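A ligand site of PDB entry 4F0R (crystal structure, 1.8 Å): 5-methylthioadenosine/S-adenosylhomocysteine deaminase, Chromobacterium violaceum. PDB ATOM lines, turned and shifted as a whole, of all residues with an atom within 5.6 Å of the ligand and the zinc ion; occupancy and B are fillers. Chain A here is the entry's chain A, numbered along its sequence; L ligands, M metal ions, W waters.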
ATOM      1  N   HIS A  70      -7.064 -19.930 -10.685  1.00  0.00           N
ATOM      2  CA  HIS A  70      -6.156 -19.978  -9.507  1.00  0.00           C
ATOM      3  C   HIS A  70      -5.769 -21.349  -9.106  1.00  0.00           C
ATOM      4  O   HIS A  70      -6.594 -22.083  -8.519  1.00  0.00           O
ATOM      5  CB  HIS A  70      -6.793 -19.238  -8.303  1.00  0.00           C
ATOM      6  CG  HIS A  70      -5.878 -19.137  -7.101  1.00  0.00           C
ATOM      7  ND1 HIS A  70      -4.780 -18.366  -7.106  1.00  0.00           N
ATOM      8  CD2 HIS A  70      -5.855 -19.831  -5.892  1.00  0.00           C
ATOM      9  CE1 HIS A  70      -4.131 -18.502  -5.938  1.00  0.00           C
ATOM     10  NE2 HIS A  70      -4.765 -19.401  -5.217  1.00  0.00           N
ATOM     11  N   HIS A  72      -2.178 -24.021  -7.786  1.00  0.00           N
ATOM     12  CA  HIS A  72      -0.796 -24.298  -7.395  1.00  0.00           C
ATOM     13  C   HIS A  72      -0.489 -25.718  -7.834  1.00  0.00           C
ATOM     14  O   HIS A  72      -0.538 -26.682  -7.031  1.00  0.00           O
ATOM     15  CB  HIS A  72      -0.613 -24.160  -5.886  1.00  0.00           C
ATOM     16  CG  HIS A  72      -1.150 -22.874  -5.324  1.00  0.00           C
ATOM     17  ND1 HIS A  72      -0.591 -21.674  -5.597  1.00  0.00           N
ATOM     18  CD2 HIS A  72      -2.261 -22.622  -4.500  1.00  0.00           C
ATOM     19  CE1 HIS A  72      -1.287 -20.703  -4.960  1.00  0.00           C
ATOM     20  NE2 HIS A  72      -2.357 -21.275  -4.355  1.00  0.00           N
ATOM     21  N   MET A  75       1.304 -28.712  -6.203  1.00  0.00           N
ATOM     22  CA  MET A  75       0.795 -29.259  -4.954  1.00  0.00           C
ATOM     23  C   MET A  75      -0.106 -30.452  -5.165  1.00  0.00           C
ATOM     24  O   MET A  75      -0.580 -31.064  -4.184  1.00  0.00           O
ATOM     25  CB  MET A  75       0.097 -28.149  -4.158  1.00  0.00           C
ATOM     26  CG  MET A  75       1.166 -27.119  -3.791  1.00  0.00           C
ATOM     27  SD  MET A  75       0.342 -25.734  -2.611  1.00  0.00           S
ATOM     28  CE  MET A  75       0.510 -26.876  -0.967  1.00  0.00           C
ATOM     29  N   LEU A  91      -0.325 -26.596   8.368  1.00  0.00           N
ATOM     30  CA  LEU A  91       0.785 -25.924   7.692  1.00  0.00           C
ATOM     31  C   LEU A  91       2.118 -26.178   8.401  1.00  0.00           C
ATOM     32  O   LEU A  91       3.096 -26.597   7.768  1.00  0.00           O
ATOM     33  CB  LEU A  91       0.513 -24.426   7.608  1.00  0.00           C
ATOM     34  CG  LEU A  91      -0.698 -24.015   6.726  1.00  0.00           C
ATOM     35  CD1 LEU A  91      -1.000 -22.547   6.948  1.00  0.00           C
ATOM     36  CD2 LEU A  91      -0.436 -24.302   5.243  1.00  0.00           C
ATOM     37  N   ILE A  95       2.434 -29.535   5.909  1.00  0.00           N
ATOM     38  CA  ILE A  95       2.658 -29.034   4.567  1.00  0.00           C
ATOM     39  C   ILE A  95       4.055 -28.392   4.401  1.00  0.00           C
ATOM     40  O   ILE A  95       4.823 -28.784   3.509  1.00  0.00           O
ATOM     41  CB  ILE A  95       1.562 -28.047   4.110  1.00  0.00           C
ATOM     42  CG1 ILE A  95       0.168 -28.734   4.071  1.00  0.00           C
ATOM     43  CG2 ILE A  95       1.950 -27.469   2.735  1.00  0.00           C
ATOM     44  CD1 ILE A  95       0.081 -29.945   3.151  1.00  0.00           C
ATOM     45  N   TRP A  96       4.425 -27.483   5.326  1.00  0.00           N
ATOM     46  CA  TRP A  96       5.680 -26.738   5.181  1.00  0.00           C
ATOM     47  C   TRP A  96       6.921 -27.603   5.350  1.00  0.00           C
ATOM     48  O   TRP A  96       7.855 -27.540   4.524  1.00  0.00           O
ATOM     49  CB  TRP A  96       5.718 -25.474   6.061  1.00  0.00           C
ATOM     50  CG  TRP A  96       4.695 -24.451   5.635  1.00  0.00           C
ATOM     51  CD1 TRP A  96       4.087 -24.314   4.375  1.00  0.00           C
ATOM     52  CD2 TRP A  96       4.079 -23.408   6.466  1.00  0.00           C
ATOM     53  NE1 TRP A  96       3.169 -23.294   4.377  1.00  0.00           N
ATOM     54  CE2 TRP A  96       3.158 -22.682   5.607  1.00  0.00           C
ATOM     55  CE3 TRP A  96       4.256 -22.998   7.783  1.00  0.00           C
ATOM     56  CZ2 TRP A  96       2.399 -21.605   6.068  1.00  0.00           C
ATOM     57  CZ3 TRP A  96       3.466 -21.937   8.250  1.00  0.00           C
ATOM     58  CH2 TRP A  96       2.570 -21.247   7.417  1.00  0.00           C
ATOM     59  N   GLU A  99       7.143 -29.573   2.036  1.00  0.00           N
ATOM     60  CA  GLU A  99       7.649 -28.695   0.977  1.00  0.00           C
ATOM     61  C   GLU A  99       9.134 -28.412   1.155  1.00  0.00           C
ATOM     62  O   GLU A  99       9.893 -28.430   0.195  1.00  0.00           O
ATOM     63  CB  GLU A  99       6.840 -27.382   0.899  1.00  0.00           C
ATOM     64  CG  GLU A  99       5.451 -27.583   0.280  1.00  0.00           C
ATOM     65  CD  GLU A  99       4.657 -26.291   0.188  1.00  0.00           C
ATOM     66  OE1 GLU A  99       4.646 -25.538   1.186  1.00  0.00           O
ATOM     67  OE2 GLU A  99       4.011 -26.053  -0.864  1.00  0.00           O
ATOM     68  N   MET A 130       0.382 -20.447  -9.723  1.00  0.00           N
ATOM     69  CA  MET A 130       1.436 -19.705  -9.050  1.00  0.00           C
ATOM     70  C   MET A 130       2.130 -20.605  -8.087  1.00  0.00           C
ATOM     71  O   MET A 130       1.521 -21.223  -7.241  1.00  0.00           O
ATOM     72  CB  MET A 130       0.992 -18.380  -8.412  1.00  0.00           C
ATOM     73  CG  MET A 130      -0.098 -18.576  -7.385  1.00  0.00           C
ATOM     74  SD  MET A 130      -0.710 -16.869  -6.595  1.00  0.00           S
ATOM     75  CE  MET A 130       0.911 -16.459  -5.523  1.00  0.00           C
ATOM     76  N   TYR A 131       3.430 -20.746  -8.298  1.00  0.00           N
ATOM     77  CA  TYR A 131       4.267 -21.590  -7.439  1.00  0.00           C
ATOM     78  C   TYR A 131       5.723 -21.137  -7.534  1.00  0.00           C
ATOM     79  O   TYR A 131       5.972 -19.974  -7.834  1.00  0.00           O
ATOM     80  CB  TYR A 131       4.094 -23.079  -7.783  1.00  0.00           C
ATOM     81  CG  TYR A 131       4.316 -23.989  -6.594  1.00  0.00           C
ATOM     82  CD1 TYR A 131       3.549 -23.846  -5.411  1.00  0.00           C
ATOM     83  CD2 TYR A 131       5.318 -24.981  -6.630  1.00  0.00           C
ATOM     84  CE1 TYR A 131       3.755 -24.695  -4.314  1.00  0.00           C
ATOM     85  CE2 TYR A 131       5.522 -25.818  -5.545  1.00  0.00           C
ATOM     86  CZ  TYR A 131       4.756 -25.681  -4.407  1.00  0.00           C
ATOM     87  OH  TYR A 131       5.005 -26.524  -3.342  1.00  0.00           O
ATOM     88  N   PHE A 132       6.654 -22.059  -7.276  1.00  0.00           N
ATOM     89  CA  PHE A 132       8.075 -21.796  -7.342  1.00  0.00           C
ATOM     90  C   PHE A 132       8.624 -22.521  -8.551  1.00  0.00           C
ATOM     91  O   PHE A 132       7.880 -23.256  -9.208  1.00  0.00           O
ATOM     92  CB  PHE A 132       8.727 -22.328  -6.064  1.00  0.00           C
ATOM     93  CG  PHE A 132       8.106 -21.789  -4.801  1.00  0.00           C
ATOM     94  CD1 PHE A 132       7.260 -22.594  -4.042  1.00  0.00           C
ATOM     95  CD2 PHE A 132       8.259 -20.439  -4.456  1.00  0.00           C
ATOM     96  CE1 PHE A 132       6.646 -22.098  -2.890  1.00  0.00           C
ATOM     97  CE2 PHE A 132       7.616 -19.937  -3.310  1.00  0.00           C
ATOM     98  CZ  PHE A 132       6.815 -20.761  -2.536  1.00  0.00           C
ATOM     99  N   SER A 153       6.162 -16.704  -8.011  1.00  0.00           N
ATOM    100  CA  SER A 153       5.787 -16.368  -6.640  1.00  0.00           C
ATOM    101  C   SER A 153       6.858 -15.549  -5.947  1.00  0.00           C
ATOM    102  O   SER A 153       8.032 -15.717  -6.195  1.00  0.00           O
ATOM    103  CB  SER A 153       5.469 -17.624  -5.826  1.00  0.00           C
ATOM    104  OG  SER A 153       4.266 -18.224  -6.310  1.00  0.00           O
ATOM    105  N   LEU A 155       7.925 -13.975  -2.085  1.00  0.00           N
ATOM    106  CA  LEU A 155       7.729 -14.125  -0.617  1.00  0.00           C
ATOM    107  C   LEU A 155       8.910 -13.378  -0.021  1.00  0.00           C
ATOM    108  O   LEU A 155       9.934 -13.179  -0.705  1.00  0.00           O
ATOM    109  CB  LEU A 155       7.868 -15.609  -0.195  1.00  0.00           C
ATOM    110  CG  LEU A 155       6.750 -16.656  -0.382  1.00  0.00           C
ATOM    111  CD1 LEU A 155       7.262 -18.046  -0.001  1.00  0.00           C
ATOM    112  CD2 LEU A 155       5.527 -16.335   0.458  1.00  0.00           C
ATOM    113  N   PHE A 157      10.442 -14.561   2.889  1.00  0.00           N
ATOM    114  CA  PHE A 157      11.313 -15.499   3.573  1.00  0.00           C
ATOM    115  C   PHE A 157      11.922 -16.531   2.633  1.00  0.00           C
ATOM    116  O   PHE A 157      11.364 -16.815   1.557  1.00  0.00           O
ATOM    117  CB  PHE A 157      10.592 -16.165   4.736  1.00  0.00           C
ATOM    118  CG  PHE A 157       9.383 -16.914   4.331  1.00  0.00           C
ATOM    119  CD1 PHE A 157       9.490 -18.224   3.834  1.00  0.00           C
ATOM    120  CD2 PHE A 157       8.132 -16.321   4.403  1.00  0.00           C
ATOM    121  CE1 PHE A 157       8.379 -18.907   3.427  1.00  0.00           C
ATOM    122  CE2 PHE A 157       6.991 -17.034   4.036  1.00  0.00           C
ATOM    123  CZ  PHE A 157       7.118 -18.314   3.515  1.00  0.00           C
ATOM    124  N   THR A 159      13.083 -20.004   0.914  1.00  0.00           N
ATOM    125  CA  THR A 159      12.623 -21.348   0.635  1.00  0.00           C
ATOM    126  C   THR A 159      13.730 -22.018  -0.175  1.00  0.00           C
ATOM    127  O   THR A 159      14.754 -21.393  -0.473  1.00  0.00           O
ATOM    128  CB  THR A 159      11.332 -21.335  -0.197  1.00  0.00           C
ATOM    129  OG1 THR A 159      11.566 -20.640  -1.443  1.00  0.00           O
ATOM    130  CG2 THR A 159      10.127 -20.658   0.603  1.00  0.00           C
ATOM    131  N   HIS A 192       2.818 -13.349  -3.011  1.00  0.00           N
ATOM    132  CA  HIS A 192       1.965 -14.351  -2.437  1.00  0.00           C
ATOM    133  C   HIS A 192       0.705 -13.817  -1.760  1.00  0.00           C
ATOM    134  O   HIS A 192      -0.409 -14.275  -2.057  1.00  0.00           O
ATOM    135  CB  HIS A 192       2.773 -15.199  -1.468  1.00  0.00           C
ATOM    136  CG  HIS A 192       1.937 -16.149  -0.700  1.00  0.00           C
ATOM    137  ND1 HIS A 192       1.679 -15.992   0.625  1.00  0.00           N
ATOM    138  CD2 HIS A 192       1.233 -17.259  -1.100  1.00  0.00           C
ATOM    139  CE1 HIS A 192       0.847 -16.944   1.037  1.00  0.00           C
ATOM    140  NE2 HIS A 192       0.580 -17.738  -0.003  1.00  0.00           N
ATOM    141  N   TYR A 195       0.199 -10.558   3.760  1.00  0.00           N
ATOM    142  CA  TYR A 195       0.867 -10.890   5.045  1.00  0.00           C
ATOM    143  C   TYR A 195       2.230 -11.545   4.877  1.00  0.00           C
ATOM    144  O   TYR A 195       2.901 -11.885   5.888  1.00  0.00           O
ATOM    145  CB  TYR A 195      -0.063 -11.772   5.919  1.00  0.00           C
ATOM    146  CG  TYR A 195      -0.587 -12.980   5.232  1.00  0.00           C
ATOM    147  CD1 TYR A 195       0.135 -14.160   5.224  1.00  0.00           C
ATOM    148  CD2 TYR A 195      -1.840 -12.962   4.642  1.00  0.00           C
ATOM    149  CE1 TYR A 195      -0.365 -15.294   4.584  1.00  0.00           C
ATOM    150  CE2 TYR A 195      -2.325 -14.066   3.965  1.00  0.00           C
ATOM    151  CZ  TYR A 195      -1.579 -15.227   3.924  1.00  0.00           C
ATOM    152  OH  TYR A 195      -2.061 -16.333   3.283  1.00  0.00           O
ATOM    153  N   THR A 196       2.670 -11.729   3.634  1.00  0.00           N
ATOM    154  CA  THR A 196       4.009 -12.341   3.360  1.00  0.00           C
ATOM    155  C   THR A 196       4.846 -11.451   2.467  1.00  0.00           C
ATOM    156  O   THR A 196       5.894 -11.863   1.978  1.00  0.00           O
ATOM    157  CB  THR A 196       3.866 -13.735   2.675  1.00  0.00           C
ATOM    158  OG1 THR A 196       2.990 -13.615   1.550  1.00  0.00           O
ATOM    159  CG2 THR A 196       3.284 -14.764   3.624  1.00  0.00           C
ATOM    160  N   HIS A 219      -2.956 -13.516  -3.547  1.00  0.00           N
ATOM    161  CA  HIS A 219      -4.055 -13.904  -2.639  1.00  0.00           C
ATOM    162  C   HIS A 219      -4.456 -12.694  -1.813  1.00  0.00           C
ATOM    163  O   HIS A 219      -3.633 -12.185  -1.050  1.00  0.00           O
ATOM    164  CB  HIS A 219      -3.588 -14.952  -1.643  1.00  0.00           C
ATOM    165  CG  HIS A 219      -3.148 -16.266  -2.272  1.00  0.00           C
ATOM    166  ND1 HIS A 219      -1.834 -16.625  -2.345  1.00  0.00           N
ATOM    167  CD2 HIS A 219      -3.882 -17.355  -2.734  1.00  0.00           C
ATOM    168  CE1 HIS A 219      -1.745 -17.867  -2.887  1.00  0.00           C
ATOM    169  NE2 HIS A 219      -2.987 -18.331  -3.108  1.00  0.00           N
ATOM    170  N   ALA A 255      -6.899 -13.350  -5.956  1.00  0.00           N
ATOM    171  CA  ALA A 255      -7.469 -14.622  -5.527  1.00  0.00           C
ATOM    172  C   ALA A 255      -8.157 -14.578  -4.170  1.00  0.00           C
ATOM    173  O   ALA A 255      -7.729 -13.883  -3.244  1.00  0.00           O
ATOM    174  CB  ALA A 255      -6.409 -15.741  -5.608  1.00  0.00           C
ATOM    175  N   HIS A 256      -9.215 -15.375  -4.062  1.00  0.00           N
ATOM    176  CA  HIS A 256     -10.048 -15.498  -2.843  1.00  0.00           C
ATOM    177  C   HIS A 256     -11.044 -14.369  -2.645  1.00  0.00           C
ATOM    178  O   HIS A 256     -12.221 -14.546  -2.889  1.00  0.00           O
ATOM    179  CB  HIS A 256      -9.217 -15.755  -1.569  1.00  0.00           C
ATOM    180  CG  HIS A 256      -8.461 -17.039  -1.614  1.00  0.00           C
ATOM    181  ND1 HIS A 256      -9.049 -18.214  -1.831  1.00  0.00           N
ATOM    182  CD2 HIS A 256      -7.082 -17.313  -1.501  1.00  0.00           C
ATOM    183  CE1 HIS A 256      -8.122 -19.207  -1.817  1.00  0.00           C
ATOM    184  NE2 HIS A 256      -6.920 -18.650  -1.655  1.00  0.00           N
ATOM    185  N   ASP A 307      -7.759 -23.620  -6.503  1.00  0.00           N
ATOM    186  CA  ASP A 307      -6.621 -23.544  -5.576  1.00  0.00           C
ATOM    187  C   ASP A 307      -5.811 -24.840  -5.718  1.00  0.00           C
ATOM    188  O   ASP A 307      -5.953 -25.578  -6.710  1.00  0.00           O
ATOM    189  CB  ASP A 307      -7.112 -23.358  -4.121  1.00  0.00           C
ATOM    190  CG  ASP A 307      -6.201 -22.443  -3.277  1.00  0.00           C
ATOM    191  OD1 ASP A 307      -5.168 -21.896  -3.765  1.00  0.00           O
ATOM    192  OD2 ASP A 307      -6.586 -22.251  -2.106  1.00  0.00           O
ATOM    193  N   GLY A 308      -4.988 -25.123  -4.725  1.00  0.00           N
ATOM    194  CA  GLY A 308      -4.116 -26.336  -4.762  1.00  0.00           C
ATOM    195  C   GLY A 308      -4.864 -27.626  -4.377  1.00  0.00           C
ATOM    196  O   GLY A 308      -5.843 -27.596  -3.601  1.00  0.00           O
HETATM  197  C1  LIG L   1       2.802 -19.704  -4.017  1.00  0.00           C
HETATM  198  S1  LIG L   1       1.658 -20.551  -3.001  1.00  0.00           S
HETATM  199  C2  LIG L   1       2.310 -20.423  -1.350  1.00  0.00           C
HETATM  200  C3  LIG L   1       3.525 -21.312  -1.207  1.00  0.00           C
HETATM  201  O1  LIG L   1       4.395 -20.805  -0.140  1.00  0.00           O
HETATM  202  C4  LIG L   1       2.968 -22.458   0.736  1.00  0.00           C
HETATM  203  O2  LIG L   1       2.955 -23.685   1.437  1.00  0.00           O
HETATM  204  C5  LIG L   1       3.052 -22.674  -0.757  1.00  0.00           C
HETATM  205  O3  LIG L   1       4.080 -23.639  -1.031  1.00  0.00           O
HETATM  206  C6  LIG L   1       4.207 -21.623   1.019  1.00  0.00           C
HETATM  207  N1  LIG L   1       4.012 -20.773   2.210  1.00  0.00           N
HETATM  208  C7  LIG L   1       3.108 -19.766   2.347  1.00  0.00           C
HETATM  209  N2  LIG L   1       3.246 -19.160   3.581  1.00  0.00           N
HETATM  210  C8  LIG L   1       4.238 -19.799   4.227  1.00  0.00           C
HETATM  211  C9  LIG L   1       4.903 -19.687   5.562  1.00  0.00           C
HETATM  212  N3  LIG L   1       4.518 -18.760   6.458  1.00  0.00           N
HETATM  213  N4  LIG L   1       5.915 -20.554   5.842  1.00  0.00           N
HETATM  214  C10 LIG L   1       6.332 -21.498   4.964  1.00  0.00           C
HETATM  215  N5  LIG L   1       5.804 -21.631   3.731  1.00  0.00           N
HETATM  216  C11 LIG L   1       4.768 -20.831   3.323  1.00  0.00           C
HETATM  217 ZN    ZN M   1      -3.906 -20.231  -3.596  1.00  0.00          ZN
HETATM  218  O   HOH W   1      -0.549 -20.077   0.443  1.00  0.00           O
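S1 of the ligand lies close to ND1 of His 72. The side-chain carboxylate (OE2) of Glu 99 sits at hydrogen-bond distance from an oxygen (O3) of the ligand (2.4 Å). O2 of the ligand is in hydrogen-bond range of NE1 of Trp 96.
The backbone carbonyl oxygen (O) of Met 130 sits at hydrogen-bond distance from a ring nitrogen (ND1) of His 72 (2.7 Å). A ring nitrogen (ND1) of His 219 lies within hydrogen-bond range of the backbone carbonyl oxygen of His 192. OE2 of Glu 99 is in hydrogen-bond range of OH of Tyr 131. The backbone carbonyl oxygen (O) of Leu 91 is in hydrogen-bond range of the backbone NH (N) of Trp 96. O of Tyr 131 sits at hydrogen-bond distance from OG of Ser 153 (2.9 Å). OG1 of Thr 196 is in hydrogen-bond range of ND1 of His 192, 2.9 Å away.
Merely in contact with the ligand: Ser 153 (3.1 Å), Phe 157 (3.3 Å), His 192 (3.4 Å), Phe 132 (3.4 Å), Tyr 131 (3.5 Å), Met 130 (3.8 Å) and Leu 155 (3.98 Å). Hydrophobic or aromatic side chains within 4 Å of the ligand: His 72, Trp 96, Tyr 131, Phe 132, Leu 155, Phe 157 and His 192.
NE2 of His 256 touches the zinc ion, 3.9 Å away. Five residues have an atom within 4 Å of the zinc ion: His 70, His 72, His 219, His 256 and Asp 307. The nearest printed residue that does not touch the zinc ion is Gly 308 (5.1 Å).
The zinc ion is bound by NE2 of His 70 (2.0 Å), NE2 of His 72 (2.0 Å), OD1 of Asp 307 (2.1 Å) and NE2 of His 219 (2.2 Å).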
